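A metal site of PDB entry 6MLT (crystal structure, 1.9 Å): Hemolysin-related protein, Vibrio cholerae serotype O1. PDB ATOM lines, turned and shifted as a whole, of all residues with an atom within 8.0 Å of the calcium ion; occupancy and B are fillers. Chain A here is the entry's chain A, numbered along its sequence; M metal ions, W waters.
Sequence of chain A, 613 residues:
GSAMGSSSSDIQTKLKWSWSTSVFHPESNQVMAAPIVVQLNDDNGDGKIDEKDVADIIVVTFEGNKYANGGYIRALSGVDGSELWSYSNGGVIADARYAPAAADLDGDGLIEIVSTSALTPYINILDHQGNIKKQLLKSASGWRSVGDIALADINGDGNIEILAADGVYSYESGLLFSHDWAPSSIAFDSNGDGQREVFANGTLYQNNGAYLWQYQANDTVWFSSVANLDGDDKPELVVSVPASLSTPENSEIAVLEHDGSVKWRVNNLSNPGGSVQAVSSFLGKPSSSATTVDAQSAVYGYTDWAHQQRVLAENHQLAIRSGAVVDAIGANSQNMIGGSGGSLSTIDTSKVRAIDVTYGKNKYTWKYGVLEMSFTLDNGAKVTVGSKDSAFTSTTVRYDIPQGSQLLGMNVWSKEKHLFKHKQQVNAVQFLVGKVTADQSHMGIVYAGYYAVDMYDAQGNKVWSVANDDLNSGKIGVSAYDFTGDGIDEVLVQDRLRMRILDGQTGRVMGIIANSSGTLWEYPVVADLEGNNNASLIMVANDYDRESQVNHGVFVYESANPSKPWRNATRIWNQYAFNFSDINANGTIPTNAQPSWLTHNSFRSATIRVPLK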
ATOM      1  N   GLN A  39      26.947  16.071   2.323  1.00  0.00           N
ATOM      2  CA  GLN A  39      27.093  17.247   1.462  1.00  0.00           C
ATOM      3  C   GLN A  39      28.504  17.816   1.557  1.00  0.00           C
ATOM      4  O   GLN A  39      28.993  18.106   2.659  1.00  0.00           O
ATOM      5  CB  GLN A  39      26.086  18.321   1.868  1.00  0.00           C
ATOM      6  CG  GLN A  39      24.624  17.910   1.859  1.00  0.00           C
ATOM      7  CD  GLN A  39      23.992  17.979   0.481  1.00  0.00           C
ATOM      8  OE1 GLN A  39      24.608  18.421  -0.483  1.00  0.00           O
ATOM      9  NE2 GLN A  39      22.743  17.541   0.393  1.00  0.00           N
ATOM     10  N   ASN A  41      29.836  20.195  -1.304  1.00  0.00           N
ATOM     11  CA  ASN A  41      30.086  21.362  -2.131  1.00  0.00           C
ATOM     12  C   ASN A  41      28.788  22.130  -2.358  1.00  0.00           C
ATOM     13  O   ASN A  41      27.687  21.651  -2.054  1.00  0.00           O
ATOM     14  CB  ASN A  41      30.740  20.987  -3.463  1.00  0.00           C
ATOM     15  CG  ASN A  41      29.777  20.328  -4.431  1.00  0.00           C
ATOM     16  OD1 ASN A  41      29.138  19.337  -4.100  1.00  0.00           O
ATOM     17  ND2 ASN A  41      29.657  20.887  -5.632  1.00  0.00           N
ATOM     18  N   ASP A  42      28.934  23.341  -2.895  1.00  0.00           N
ATOM     19  CA  ASP A  42      27.810  24.237  -3.126  1.00  0.00           C
ATOM     20  C   ASP A  42      27.317  24.021  -4.553  1.00  0.00           C
ATOM     21  O   ASP A  42      27.814  24.642  -5.500  1.00  0.00           O
ATOM     22  CB  ASP A  42      28.217  25.674  -2.876  1.00  0.00           C
ATOM     23  CG  ASP A  42      27.073  26.650  -3.060  1.00  0.00           C
ATOM     24  OD1 ASP A  42      25.907  26.204  -3.110  1.00  0.00           O
ATOM     25  OD2 ASP A  42      27.352  27.861  -3.167  1.00  0.00           O
ATOM     26  N   ASP A  43      26.345  23.129  -4.718  1.00  0.00           N
ATOM     27  CA  ASP A  43      25.852  22.804  -6.061  1.00  0.00           C
ATOM     28  C   ASP A  43      24.979  23.915  -6.633  1.00  0.00           C
ATOM     29  O   ASP A  43      25.069  24.216  -7.827  1.00  0.00           O
ATOM     30  CB  ASP A  43      25.075  21.494  -6.028  1.00  0.00           C
ATOM     31  CG  ASP A  43      25.967  20.296  -5.812  1.00  0.00           C
ATOM     32  OD1 ASP A  43      26.761  19.979  -6.714  1.00  0.00           O
ATOM     33  OD2 ASP A  43      25.879  19.690  -4.731  1.00  0.00           O
ATOM     34  N   ASN A  44      24.107  24.520  -5.824  1.00  0.00           N
ATOM     35  CA  ASN A  44      23.192  25.541  -6.323  1.00  0.00           C
ATOM     36  C   ASN A  44      23.767  26.952  -6.287  1.00  0.00           C
ATOM     37  O   ASN A  44      23.069  27.898  -6.648  1.00  0.00           O
ATOM     38  CB  ASN A  44      21.874  25.505  -5.543  1.00  0.00           C
ATOM     39  CG  ASN A  44      22.034  25.888  -4.088  1.00  0.00           C
ATOM     40  OD1 ASN A  44      23.111  26.309  -3.659  1.00  0.00           O
ATOM     41  ND2 ASN A  44      20.962  25.759  -3.330  1.00  0.00           N
ATOM     42  N   GLY A  45      25.020  27.114  -5.857  1.00  0.00           N
ATOM     43  CA  GLY A  45      25.696  28.395  -5.941  1.00  0.00           C
ATOM     44  C   GLY A  45      25.109  29.492  -5.083  1.00  0.00           C
ATOM     45  O   GLY A  45      25.163  30.665  -5.469  1.00  0.00           O
ATOM     46  N   ASP A  46      24.559  29.163  -3.916  1.00  0.00           N
ATOM     47  CA  ASP A  46      24.019  30.159  -3.010  1.00  0.00           C
ATOM     48  C   ASP A  46      24.971  30.497  -1.868  1.00  0.00           C
ATOM     49  O   ASP A  46      24.564  31.121  -0.891  1.00  0.00           O
ATOM     50  CB  ASP A  46      22.677  29.684  -2.433  1.00  0.00           C
ATOM     51  CG  ASP A  46      22.814  28.465  -1.550  1.00  0.00           C
ATOM     52  OD1 ASP A  46      23.926  27.903  -1.446  1.00  0.00           O
ATOM     53  OD2 ASP A  46      21.790  28.068  -0.937  1.00  0.00           O
ATOM     54  N   GLY A  47      26.242  30.107  -1.985  1.00  0.00           N
ATOM     55  CA  GLY A  47      27.231  30.411  -0.968  1.00  0.00           C
ATOM     56  C   GLY A  47      27.192  29.538   0.256  1.00  0.00           C
ATOM     57  O   GLY A  47      28.005  29.750   1.172  1.00  0.00           O
ATOM     58  N   LYS A  48      26.284  28.565   0.314  1.00  0.00           N
ATOM     59  CA  LYS A  48      26.145  27.681   1.459  1.00  0.00           C
ATOM     60  C   LYS A  48      26.215  26.237   0.991  1.00  0.00           C
ATOM     61  O   LYS A  48      25.968  25.930  -0.182  1.00  0.00           O
ATOM     62  CB  LYS A  48      24.821  27.929   2.195  1.00  0.00           C
ATOM     63  N   ILE A  49      26.559  25.357   1.919  1.00  0.00           N
ATOM     64  CA  ILE A  49      26.526  23.917   1.682  1.00  0.00           C
ATOM     65  C   ILE A  49      25.554  23.320   2.685  1.00  0.00           C
ATOM     66  O   ILE A  49      25.860  23.214   3.881  1.00  0.00           O
ATOM     67  CB  ILE A  49      27.915  23.275   1.813  1.00  0.00           C
ATOM     68  CG1 ILE A  49      28.874  23.924   0.801  1.00  0.00           C
ATOM     69  CG2 ILE A  49      27.828  21.779   1.576  1.00  0.00           C
ATOM     70  CD1 ILE A  49      30.306  23.459   0.914  1.00  0.00           C
ATOM     71  N   ASP A  50      24.373  22.931   2.216  1.00  0.00           N
ATOM     72  CA  ASP A  50      23.347  22.385   3.092  1.00  0.00           C
ATOM     73  C   ASP A  50      22.468  21.435   2.288  1.00  0.00           C
ATOM     74  O   ASP A  50      22.809  21.038   1.164  1.00  0.00           O
ATOM     75  CB  ASP A  50      22.544  23.516   3.753  1.00  0.00           C
ATOM     76  CG  ASP A  50      21.868  24.419   2.757  1.00  0.00           C
ATOM     77  OD1 ASP A  50      21.653  23.989   1.600  1.00  0.00           O
ATOM     78  OD2 ASP A  50      21.557  25.567   3.120  1.00  0.00           O
ATOM     79  N   GLU A  51      21.316  21.074   2.855  1.00  0.00           N
ATOM     80  CA  GLU A  51      20.435  20.065   2.257  1.00  0.00           C
ATOM     81  C   GLU A  51      19.809  20.509   0.940  1.00  0.00           C
ATOM     82  O   GLU A  51      19.205  19.678   0.258  1.00  0.00           O
ATOM     83  CB  GLU A  51      19.334  19.662   3.240  1.00  0.00           C
ATOM     84  CG  GLU A  51      18.591  20.807   3.904  1.00  0.00           C
ATOM     85  CD  GLU A  51      19.114  21.122   5.292  1.00  0.00           C
ATOM     86  OE1 GLU A  51      20.239  21.671   5.396  1.00  0.00           O
ATOM     87  OE2 GLU A  51      18.422  20.809   6.279  1.00  0.00           O
ATOM     88  N   LYS A  52      19.955  21.774   0.556  1.00  0.00           N
ATOM     89  CA  LYS A  52      19.500  22.179  -0.763  1.00  0.00           C
ATOM     90  C   LYS A  52      20.465  21.733  -1.857  1.00  0.00           C
ATOM     91  O   LYS A  52      20.097  21.731  -3.032  1.00  0.00           O
ATOM     92  CB  LYS A  52      19.322  23.699  -0.819  1.00  0.00           C
ATOM     93  N   ASP A  53      21.681  21.332  -1.495  1.00  0.00           N
ATOM     94  CA  ASP A  53      22.657  20.861  -2.462  1.00  0.00           C
ATOM     95  C   ASP A  53      22.489  19.358  -2.668  1.00  0.00           C
ATOM     96  O   ASP A  53      21.626  18.711  -2.070  1.00  0.00           O
ATOM     97  CB  ASP A  53      24.062  21.233  -2.000  1.00  0.00           C
ATOM     98  CG  ASP A  53      24.240  22.724  -1.869  1.00  0.00           C
ATOM     99  OD1 ASP A  53      24.116  23.428  -2.891  1.00  0.00           O
ATOM    100  OD2 ASP A  53      24.476  23.201  -0.738  1.00  0.00           O
ATOM    101  N   VAL A  54      23.331  18.786  -3.528  1.00  0.00           N
ATOM    102  CA  VAL A  54      23.268  17.368  -3.869  1.00  0.00           C
ATOM    103  C   VAL A  54      24.297  16.628  -3.043  1.00  0.00           C
ATOM    104  O   VAL A  54      25.501  16.905  -3.150  1.00  0.00           O
ATOM    105  CB  VAL A  54      23.480  17.150  -5.373  1.00  0.00           C
ATOM    106  CG1 VAL A  54      23.403  15.663  -5.724  1.00  0.00           C
ATOM    107  CG2 VAL A  54      22.461  17.922  -6.175  1.00  0.00           C
HETATM  108 CA    CA M   1      24.310  25.583  -1.729  1.00  0.00          CA
HETATM  109  O   HOH W   1      22.383  25.612  -0.588  1.00  0.00           O
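The backbone NH of Gly 47 lies within hydrogen-bond range of the side-chain carboxylate of Asp 42, at 2.8 Å. N of Gly 45 lies close to OD1 of Asp 42, at 3.0 Å. The backbone carbonyl oxygen (O) of Asp 53 lies within hydrogen-bond range of the side-chain amide nitrogen (NE2) of Gln 39, at 2.9 Å. OD1 of Asp 53 lies close to N of Asp 43 (2.9 Å). N of Asp 50 lies close to OD2 of Asp 53.
Water W1 lies within hydrogen-bond range of OD2 of Asp 46 (2.6 Å), OD1 of Asp 50 (2.8 Å) and ND2 of Asn 44 (3.1 Å).
Within 4 Å of the calcium ion: Asp 42, Asn 44, Asp 46, Lys 48 and Asp 53.
The calcium ion is bound by OD1 of Asp 42, water W1, O of Lys 48, OD1 of Asp 46, OD1 of Asn 44, OD1 of Asp 53 and OD2 of Asp 53.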
